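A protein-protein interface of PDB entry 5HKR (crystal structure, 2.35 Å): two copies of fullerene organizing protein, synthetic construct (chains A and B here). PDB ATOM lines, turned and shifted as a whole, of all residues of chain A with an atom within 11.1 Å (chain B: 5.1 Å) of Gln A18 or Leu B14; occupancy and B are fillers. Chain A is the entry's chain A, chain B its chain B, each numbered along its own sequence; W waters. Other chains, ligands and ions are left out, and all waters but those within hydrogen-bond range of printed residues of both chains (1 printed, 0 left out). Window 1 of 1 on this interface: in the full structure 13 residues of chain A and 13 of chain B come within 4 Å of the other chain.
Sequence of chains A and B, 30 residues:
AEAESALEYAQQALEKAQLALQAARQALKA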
ATOM      1  N   TYR A   9      24.868  -7.471  14.343  1.00  0.00           N
ATOM      2  CA  TYR A   9      24.631  -7.508  12.907  1.00  0.00           C
ATOM      3  C   TYR A   9      24.774  -8.923  12.360  1.00  0.00           C
ATOM      4  O   TYR A   9      23.943  -9.379  11.570  1.00  0.00           O
ATOM      5  CB  TYR A   9      25.601  -6.550  12.219  1.00  0.00           C
ATOM      6  CG  TYR A   9      25.592  -6.535  10.706  1.00  0.00           C
ATOM      7  CD1 TYR A   9      26.289  -7.491   9.967  1.00  0.00           C
ATOM      8  CD2 TYR A   9      24.933  -5.530  10.011  1.00  0.00           C
ATOM      9  CE1 TYR A   9      26.300  -7.457   8.585  1.00  0.00           C
ATOM     10  CE2 TYR A   9      24.937  -5.492   8.627  1.00  0.00           C
ATOM     11  CZ  TYR A   9      25.625  -6.451   7.926  1.00  0.00           C
ATOM     12  OH  TYR A   9      25.630  -6.393   6.562  1.00  0.00           O
ATOM     13  N   ALA A  10      25.824  -9.634  12.764  1.00  0.00           N
ATOM     14  CA  ALA A  10      26.014 -10.986  12.256  1.00  0.00           C
ATOM     15  C   ALA A  10      24.874 -11.891  12.672  1.00  0.00           C
ATOM     16  O   ALA A  10      24.513 -12.811  11.933  1.00  0.00           O
ATOM     17  CB  ALA A  10      27.344 -11.561  12.738  1.00  0.00           C
ATOM     18  N   GLN A  11      24.285 -11.645  13.838  1.00  0.00           N
ATOM     19  CA  GLN A  11      23.110 -12.412  14.227  1.00  0.00           C
ATOM     20  C   GLN A  11      21.936 -12.094  13.311  1.00  0.00           C
ATOM     21  O   GLN A  11      21.256 -13.005  12.820  1.00  0.00           O
ATOM     22  CB  GLN A  11      22.761 -12.134  15.682  1.00  0.00           C
ATOM     23  CG  GLN A  11      21.758 -13.104  16.255  1.00  0.00           C
ATOM     24  CD  GLN A  11      21.651 -12.981  17.756  1.00  0.00           C
ATOM     25  OE1 GLN A  11      20.695 -12.396  18.277  1.00  0.00           O
ATOM     26  NE2 GLN A  11      22.632 -13.530  18.465  1.00  0.00           N
ATOM     27  N   GLN A  12      21.695 -10.804  13.062  1.00  0.00           N
ATOM     28  CA  GLN A  12      20.737 -10.388  12.041  1.00  0.00           C
ATOM     29  C   GLN A  12      20.924 -11.184  10.759  1.00  0.00           C
ATOM     30  O   GLN A  12      20.004 -11.866  10.293  1.00  0.00           O
ATOM     31  CB  GLN A  12      20.895  -8.892  11.757  1.00  0.00           C
ATOM     32  CG  GLN A  12      20.161  -8.417  10.503  1.00  0.00           C
ATOM     33  CD  GLN A  12      20.916  -7.343   9.702  1.00  0.00           C
ATOM     34  OE1 GLN A  12      21.797  -7.651   8.883  1.00  0.00           O
ATOM     35  NE2 GLN A  12      20.549  -6.083   9.918  1.00  0.00           N
ATOM     36  N   ALA A  13      22.125 -11.105  10.177  1.00  0.00           N
ATOM     37  CA  ALA A  13      22.417 -11.822   8.939  1.00  0.00           C
ATOM     38  C   ALA A  13      22.084 -13.303   9.055  1.00  0.00           C
ATOM     39  O   ALA A  13      21.479 -13.882   8.148  1.00  0.00           O
ATOM     40  CB  ALA A  13      23.886 -11.635   8.565  1.00  0.00           C
ATOM     41  N   LEU A  14      22.464 -13.928  10.170  1.00  0.00           N
ATOM     42  CA  LEU A  14      22.172 -15.344  10.364  1.00  0.00           C
ATOM     43  C   LEU A  14      20.678 -15.616  10.379  1.00  0.00           C
ATOM     44  O   LEU A  14      20.216 -16.607   9.805  1.00  0.00           O
ATOM     45  CB  LEU A  14      22.796 -15.835  11.663  1.00  0.00           C
ATOM     46  CG  LEU A  14      24.308 -15.972  11.622  1.00  0.00           C
ATOM     47  CD1 LEU A  14      24.788 -16.696  12.875  1.00  0.00           C
ATOM     48  CD2 LEU A  14      24.701 -16.708  10.351  1.00  0.00           C
ATOM     49  N   GLU A  15      19.904 -14.751  11.035  1.00  0.00           N
ATOM     50  CA  GLU A  15      18.461 -14.948  11.049  1.00  0.00           C
ATOM     51  C   GLU A  15      17.854 -14.689   9.674  1.00  0.00           C
ATOM     52  O   GLU A  15      16.957 -15.426   9.253  1.00  0.00           O
ATOM     53  CB  GLU A  15      17.830 -14.077  12.135  1.00  0.00           C
ATOM     54  CG  GLU A  15      18.529 -14.282  13.494  1.00  0.00           C
ATOM     55  CD  GLU A  15      18.106 -13.289  14.560  1.00  0.00           C
ATOM     56  OE1 GLU A  15      18.050 -13.681  15.749  1.00  0.00           O
ATOM     57  OE2 GLU A  15      17.830 -12.128  14.194  1.00  0.00           O
ATOM     58  N   LYS A  16      18.335 -13.668   8.951  1.00  0.00           N
ATOM     59  CA  LYS A  16      17.913 -13.502   7.560  1.00  0.00           C
ATOM     60  C   LYS A  16      18.191 -14.770   6.774  1.00  0.00           C
ATOM     61  O   LYS A  16      17.350 -15.232   5.996  1.00  0.00           O
ATOM     62  CB  LYS A  16      18.625 -12.310   6.895  1.00  0.00           C
ATOM     63  CG  LYS A  16      18.502 -10.948   7.611  1.00  0.00           C
ATOM     64  CD  LYS A  16      18.968  -9.734   6.747  1.00  0.00           C
ATOM     65  CE  LYS A  16      20.453  -9.779   6.300  1.00  0.00           C
ATOM     66  NZ  LYS A  16      21.264  -8.537   6.652  1.00  0.00           N
ATOM     67  N   ALA A  17      19.369 -15.358   6.982  1.00  0.00           N
ATOM     68  CA  ALA A  17      19.743 -16.554   6.242  1.00  0.00           C
ATOM     69  C   ALA A  17      18.798 -17.706   6.540  1.00  0.00           C
ATOM     70  O   ALA A  17      18.403 -18.445   5.631  1.00  0.00           O
ATOM     71  CB  ALA A  17      21.181 -16.943   6.578  1.00  0.00           C
ATOM     72  N   GLN A  18      18.419 -17.880   7.807  1.00  0.00           N
ATOM     73  CA  GLN A  18      17.609 -19.042   8.143  1.00  0.00           C
ATOM     74  C   GLN A  18      16.206 -18.941   7.566  1.00  0.00           C
ATOM     75  O   GLN A  18      15.595 -19.968   7.261  1.00  0.00           O
ATOM     76  CB  GLN A  18      17.578 -19.245   9.652  1.00  0.00           C
ATOM     77  CG  GLN A  18      18.879 -19.840  10.157  1.00  0.00           C
ATOM     78  CD  GLN A  18      18.731 -20.580  11.472  1.00  0.00           C
ATOM     79  OE1 GLN A  18      18.237 -20.025  12.455  1.00  0.00           O
ATOM     80  NE2 GLN A  18      19.150 -21.846  11.493  1.00  0.00           N
ATOM     81  N   LEU A  19      15.686 -17.726   7.396  1.00  0.00           N
ATOM     82  CA  LEU A  19      14.482 -17.557   6.591  1.00  0.00           C
ATOM     83  C   LEU A  19      14.675 -18.172   5.219  1.00  0.00           C
ATOM     84  O   LEU A  19      13.875 -18.998   4.766  1.00  0.00           O
ATOM     85  CB  LEU A  19      14.155 -16.077   6.424  1.00  0.00           C
ATOM     86  CG  LEU A  19      14.056 -15.164   7.625  1.00  0.00           C
ATOM     87  CD1 LEU A  19      14.223 -13.740   7.164  1.00  0.00           C
ATOM     88  CD2 LEU A  19      12.715 -15.353   8.228  1.00  0.00           C
ATOM     89  N   ALA A  20      15.750 -17.761   4.544  1.00  0.00           N
ATOM     90  CA  ALA A  20      16.008 -18.204   3.181  1.00  0.00           C
ATOM     91  C   ALA A  20      16.058 -19.723   3.093  1.00  0.00           C
ATOM     92  O   ALA A  20      15.523 -20.317   2.151  1.00  0.00           O
ATOM     93  CB  ALA A  20      17.315 -17.580   2.685  1.00  0.00           C
ATOM     94  N   LEU A  21      16.686 -20.368   4.073  1.00  0.00           N
ATOM     95  CA  LEU A  21      16.768 -21.821   4.071  1.00  0.00           C
ATOM     96  C   LEU A  21      15.393 -22.450   4.130  1.00  0.00           C
ATOM     97  O   LEU A  21      15.041 -23.276   3.284  1.00  0.00           O
ATOM     98  CB  LEU A  21      17.599 -22.299   5.252  1.00  0.00           C
ATOM     99  CG  LEU A  21      19.045 -21.859   5.208  1.00  0.00           C
ATOM    100  CD1 LEU A  21      19.798 -22.521   6.340  1.00  0.00           C
ATOM    101  CD2 LEU A  21      19.621 -22.243   3.856  1.00  0.00           C
ATOM    102  N   GLN A  22      14.603 -22.083   5.140  1.00  0.00           N
ATOM    103  CA  GLN A  22      13.329 -22.759   5.333  1.00  0.00           C
ATOM    104  C   GLN A  22      12.446 -22.600   4.110  1.00  0.00           C
ATOM    105  O   GLN A  22      11.774 -23.548   3.699  1.00  0.00           O
ATOM    106  CB  GLN A  22      12.631 -22.235   6.584  1.00  0.00           C
ATOM    107  CG  GLN A  22      13.463 -22.386   7.842  1.00  0.00           C
ATOM    108  CD  GLN A  22      14.069 -23.774   8.015  1.00  0.00           C
ATOM    109  OE1 GLN A  22      15.239 -23.909   8.394  1.00  0.00           O
ATOM    110  NE2 GLN A  22      13.274 -24.808   7.767  1.00  0.00           N
ATOM    111  N   ALA A  23      12.451 -21.414   3.503  1.00  0.00           N
ATOM    112  CA  ALA A  23      11.758 -21.244   2.236  1.00  0.00           C
ATOM    113  C   ALA A  23      12.312 -22.210   1.202  1.00  0.00           C
ATOM    114  O   ALA A  23      11.559 -22.921   0.530  1.00  0.00           O
ATOM    115  CB  ALA A  23      11.879 -19.797   1.756  1.00  0.00           C
ATOM    116  N   ALA A  24      13.638 -22.275   1.090  1.00  0.00           N
ATOM    117  CA  ALA A  24      14.239 -23.200   0.138  1.00  0.00           C
ATOM    118  C   ALA A  24      13.894 -24.641   0.486  1.00  0.00           C
ATOM    119  O   ALA A  24      13.617 -25.455  -0.406  1.00  0.00           O
ATOM    120  CB  ALA A  24      15.751 -23.003   0.094  1.00  0.00           C
ATOM    121  N   ARG A  25      13.888 -24.973   1.779  1.00  0.00           N
ATOM    122  CA  ARG A  25      13.544 -26.330   2.186  1.00  0.00           C
ATOM    123  C   ARG A  25      12.129 -26.688   1.760  1.00  0.00           C
ATOM    124  O   ARG A  25      11.890 -27.785   1.242  1.00  0.00           O
ATOM    125  CB  ARG A  25      13.710 -26.488   3.695  1.00  0.00           C
ATOM    126  CG  ARG A  25      15.112 -26.233   4.143  1.00  0.00           C
ATOM    127  CD  ARG A  25      15.711 -27.470   4.722  1.00  0.00           C
ATOM    128  NE  ARG A  25      15.582 -27.557   6.171  1.00  0.00           N
ATOM    129  CZ  ARG A  25      15.481 -28.712   6.818  1.00  0.00           C
ATOM    130  NH1 ARG A  25      15.469 -29.842   6.127  1.00  0.00           N
ATOM    131  NH2 ARG A  25      15.384 -28.738   8.144  1.00  0.00           N
ATOM    132  N   GLN A  26      11.180 -25.771   1.950  1.00  0.00           N
ATOM    133  CA  GLN A  26       9.811 -26.036   1.516  1.00  0.00           C
ATOM    134  C   GLN A  26       9.736 -26.200   0.002  1.00  0.00           C
ATOM    135  O   GLN A  26       9.074 -27.112  -0.505  1.00  0.00           O
ATOM    136  CB  GLN A  26       8.878 -24.918   1.984  1.00  0.00           C
ATOM    137  CG  GLN A  26       7.472 -25.012   1.385  1.00  0.00           C
ATOM    138  CD  GLN A  26       6.686 -26.218   1.876  1.00  0.00           C
ATOM    139  OE1 GLN A  26       6.673 -26.522   3.069  1.00  0.00           O
ATOM    140  NE2 GLN A  26       6.035 -26.916   0.954  1.00  0.00           N
ATOM    141  N   ALA A  27      10.418 -25.326  -0.739  1.00  0.00           N
ATOM    142  CA  ALA A  27      10.403 -25.444  -2.189  1.00  0.00           C
ATOM    143  C   ALA A  27      10.892 -26.810  -2.641  1.00  0.00           C
ATOM    144  O   ALA A  27      10.408 -27.336  -3.647  1.00  0.00           O
ATOM    145  CB  ALA A  27      11.246 -24.337  -2.812  1.00  0.00           C
ATOM    146  N   ALA B  10      22.843 -27.561   6.285  1.00  0.00           N
ATOM    147  CA  ALA B  10      23.126 -26.138   6.414  1.00  0.00           C
ATOM    148  C   ALA B  10      22.334 -25.524   7.554  1.00  0.00           C
ATOM    149  O   ALA B  10      22.882 -24.758   8.352  1.00  0.00           O
ATOM    150  CB  ALA B  10      22.824 -25.420   5.102  1.00  0.00           C
ATOM    151  N   GLN B  11      21.046 -25.857   7.659  1.00  0.00           N
ATOM    152  CA  GLN B  11      20.224 -25.279   8.719  1.00  0.00           C
ATOM    153  C   GLN B  11      20.777 -25.629  10.093  1.00  0.00           C
ATOM    154  O   GLN B  11      20.832 -24.776  10.987  1.00  0.00           O
ATOM    155  CB  GLN B  11      18.785 -25.763   8.588  1.00  0.00           C
ATOM    156  CG  GLN B  11      17.917 -25.413   9.779  1.00  0.00           C
ATOM    157  CD  GLN B  11      16.670 -26.281   9.872  1.00  0.00           C
ATOM    158  OE1 GLN B  11      16.077 -26.647   8.854  1.00  0.00           O
ATOM    159  NE2 GLN B  11      16.271 -26.623  11.100  1.00  0.00           N
ATOM    160  N   GLN B  12      21.208 -26.877  10.273  1.00  0.00           N
ATOM    161  CA  GLN B  12      21.833 -27.276  11.528  1.00  0.00           C
ATOM    162  C   GLN B  12      23.066 -26.439  11.819  1.00  0.00           C
ATOM    163  O   GLN B  12      23.231 -25.923  12.927  1.00  0.00           O
ATOM    164  CB  GLN B  12      22.217 -28.748  11.479  1.00  0.00           C
ATOM    165  CG  GLN B  12      21.059 -29.677  11.325  1.00  0.00           C
ATOM    166  CD  GLN B  12      21.507 -31.109  11.189  1.00  0.00           C
ATOM    167  OE1 GLN B  12      22.669 -31.435  11.448  1.00  0.00           O
ATOM    168  NE2 GLN B  12      20.594 -31.977  10.775  1.00  0.00           N
ATOM    169  N   ALA B  13      23.956 -26.316  10.833  1.00  0.00           N
ATOM    170  CA  ALA B  13      25.202 -25.587  11.042  1.00  0.00           C
ATOM    171  C   ALA B  13      24.932 -24.162  11.503  1.00  0.00           C
ATOM    172  O   ALA B  13      25.649 -23.631  12.361  1.00  0.00           O
ATOM    173  CB  ALA B  13      26.035 -25.599   9.760  1.00  0.00           C
ATOM    174  N   LEU B  14      23.885 -23.532  10.969  1.00  0.00           N
ATOM    175  CA  LEU B  14      23.571 -22.169  11.379  1.00  0.00           C
ATOM    176  C   LEU B  14      23.126 -22.112  12.827  1.00  0.00           C
ATOM    177  O   LEU B  14      23.446 -21.156  13.538  1.00  0.00           O
ATOM    178  CB  LEU B  14      22.492 -21.575  10.489  1.00  0.00           C
ATOM    179  CG  LEU B  14      22.986 -21.150   9.116  1.00  0.00           C
ATOM    180  CD1 LEU B  14      22.079 -20.053   8.587  1.00  0.00           C
ATOM    181  CD2 LEU B  14      24.438 -20.690   9.175  1.00  0.00           C
ATOM    182  N   GLU B  15      22.377 -23.119  13.275  1.00  0.00           N
ATOM    183  CA  GLU B  15      21.958 -23.158  14.671  1.00  0.00           C
ATOM    184  C   GLU B  15      23.165 -23.262  15.594  1.00  0.00           C
ATOM    185  O   GLU B  15      23.266 -22.530  16.590  1.00  0.00           O
ATOM    186  CB  GLU B  15      20.980 -24.315  14.878  1.00  0.00           C
ATOM    187  CG  GLU B  15      19.767 -24.191  13.971  1.00  0.00           C
ATOM    188  CD  GLU B  15      18.698 -25.235  14.227  1.00  0.00           C
ATOM    189  OE1 GLU B  15      18.959 -26.160  15.027  1.00  0.00           O
ATOM    190  OE2 GLU B  15      17.598 -25.129  13.621  1.00  0.00           O
ATOM    191  N   LYS B  16      24.110 -24.144  15.258  1.00  0.00           N
ATOM    192  CA  LYS B  16      25.358 -24.203  16.008  1.00  0.00           C
ATOM    193  C   LYS B  16      26.102 -22.880  15.912  1.00  0.00           C
ATOM    194  O   LYS B  16      26.701 -22.421  16.889  1.00  0.00           O
ATOM    195  CB  LYS B  16      26.212 -25.356  15.487  1.00  0.00           C
ATOM    196  CG  LYS B  16      25.539 -26.727  15.601  1.00  0.00           C
ATOM    197  CD  LYS B  16      26.235 -27.757  14.709  1.00  0.00           C
ATOM    198  CE  LYS B  16      25.886 -29.190  15.075  1.00  0.00           C
ATOM    199  NZ  LYS B  16      26.956 -29.802  15.903  1.00  0.00           N
ATOM    200  N   ALA B  17      26.065 -22.242  14.744  1.00  0.00           N
ATOM    201  CA  ALA B  17      26.642 -20.910  14.638  1.00  0.00           C
ATOM    202  C   ALA B  17      25.861 -19.911  15.482  1.00  0.00           C
ATOM    203  O   ALA B  17      26.446 -19.009  16.088  1.00  0.00           O
ATOM    204  CB  ALA B  17      26.687 -20.475  13.176  1.00  0.00           C
ATOM    205  N   GLN B  18      24.541 -20.077  15.563  1.00  0.00           N
ATOM    206  CA  GLN B  18      23.726 -19.129  16.313  1.00  0.00           C
ATOM    207  C   GLN B  18      23.951 -19.251  17.814  1.00  0.00           C
ATOM    208  O   GLN B  18      24.211 -18.252  18.493  1.00  0.00           O
ATOM    209  CB  GLN B  18      22.257 -19.334  15.979  1.00  0.00           C
ATOM    210  CG  GLN B  18      21.849 -18.694  14.683  1.00  0.00           C
ATOM    211  CD  GLN B  18      20.574 -19.287  14.148  1.00  0.00           C
ATOM    212  OE1 GLN B  18      20.429 -20.510  14.085  1.00  0.00           O
ATOM    213  NE2 GLN B  18      19.629 -18.426  13.766  1.00  0.00           N
ATOM    214  N   LEU B  19      23.839 -20.462  18.360  1.00  0.00           N
ATOM    215  CA  LEU B  19      23.915 -20.608  19.813  1.00  0.00           C
ATOM    216  C   LEU B  19      25.301 -20.254  20.339  1.00  0.00           C
ATOM    217  O   LEU B  19      25.435 -19.688  21.430  1.00  0.00           O
ATOM    218  CB  LEU B  19      23.510 -22.029  20.219  1.00  0.00           C
ATOM    219  CG  LEU B  19      24.337 -23.258  19.810  1.00  0.00           C
ATOM    220  CD1 LEU B  19      25.544 -23.453  20.705  1.00  0.00           C
ATOM    221  CD2 LEU B  19      23.484 -24.522  19.825  1.00  0.00           C
HETATM  222  O   HOH W   1      16.878 -17.942  13.251  1.00  0.00           O
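The backbone carbonyl oxygen (O) of Gln B11 sits at hydrogen-bond distance from the side-chain amide nitrogen (NE2) of Gln A18, at 3.4 Å. OE1 of Gln A18 is in hydrogen-bond range of NE2 of Gln B18 (2.5 Å). The side-chain amide oxygen (OE1) of Gln B11 lies close to the side-chain amide oxygen (OE1) of Gln A22. OE1 of Gln B11 sits at hydrogen-bond distance from NE of Arg A25 (2.9 Å).
The side-chain amide nitrogen of Gln B11 is in hydrogen-bond range of the side-chain carboxylate of Glu B15, 3.2 Å away. O of Leu B14 lies close to OE1 of Gln B18, at 3.1 Å. The side-chain amide oxygen of Gln B18 lies close to the backbone NH of Glu B15 (3.4 Å).
Among the printed residues, merely in contact across the chains: Leu A14 with Gln B18 (3.99 Å), Ala A17 with Leu B14 (3.8 Å), Gln A18 with Leu B14 (3.5 Å), Gln A18 with Glu B15 (3.5 Å) and Leu A21 with Gln B11 (3.7 Å).
Printed residues of chain B within 4 Å of Ala A17: Leu B14 (3.8 Å). Of the printed residues of chain B, Leu A21 touches Gln B11. Printed residues of chain B within 4 Å of Arg A25: Gln B11. Ala A27 touches none of the printed residues of chain B. No residue of chain A comes within 4 Å of Ala B10. Of chain A, only Gln A18 (3.4 Å), Leu A21 (3.7 Å), Gln A22 (2.9 Å) and Arg A25 (2.3 Å) come within 4 Å of Gln B11. No residue of chain A comes within 4 Å of Ala B13. Of chain A, only Ala A17 (3.8 Å) and Gln A18 (3.5 Å) come within 4 Å of Leu B14. The nearest printed residue of chain B that does not touch Gln A18 is Gln B12 (5.6 Å). The nearest printed residue of chain B that does not touch Gln A22 is Glu B15 (5.9 Å).
Of the 10 printed residues of chain B, 4 touch a printed residue of chain A. Printed residues of chain A that touch a printed residue of chain B: Leu A14, Ala A17, Gln A18, Leu A21, Gln A22 and Arg A25. Hydrophobic or aromatic side chains of chain A that line the printed part of chain B: Leu A14, Ala A17 and Leu A21. Along chain A the printed residues that touch a printed residue of chain B span positions 14 to 25.
Ala A17 touches Leu B14, but with the chains exchanged Leu A14 does not touch Ala B17 (4.2 Å). Gln A18 touches Gln B11, but with the chains exchanged Gln A11 does not touch Gln B18 (5.0 Å). Gln A18 touches Glu B15, but with the chains exchanged Glu A15 does not touch Gln B18 (4.3 Å). Gln B18 touches its own counterpart, Gln A18.
Water W1 lies within hydrogen-bond range of OE1 of Gln A18 (2.6 Å) and NE2 of Gln B18 (2.8 Å).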
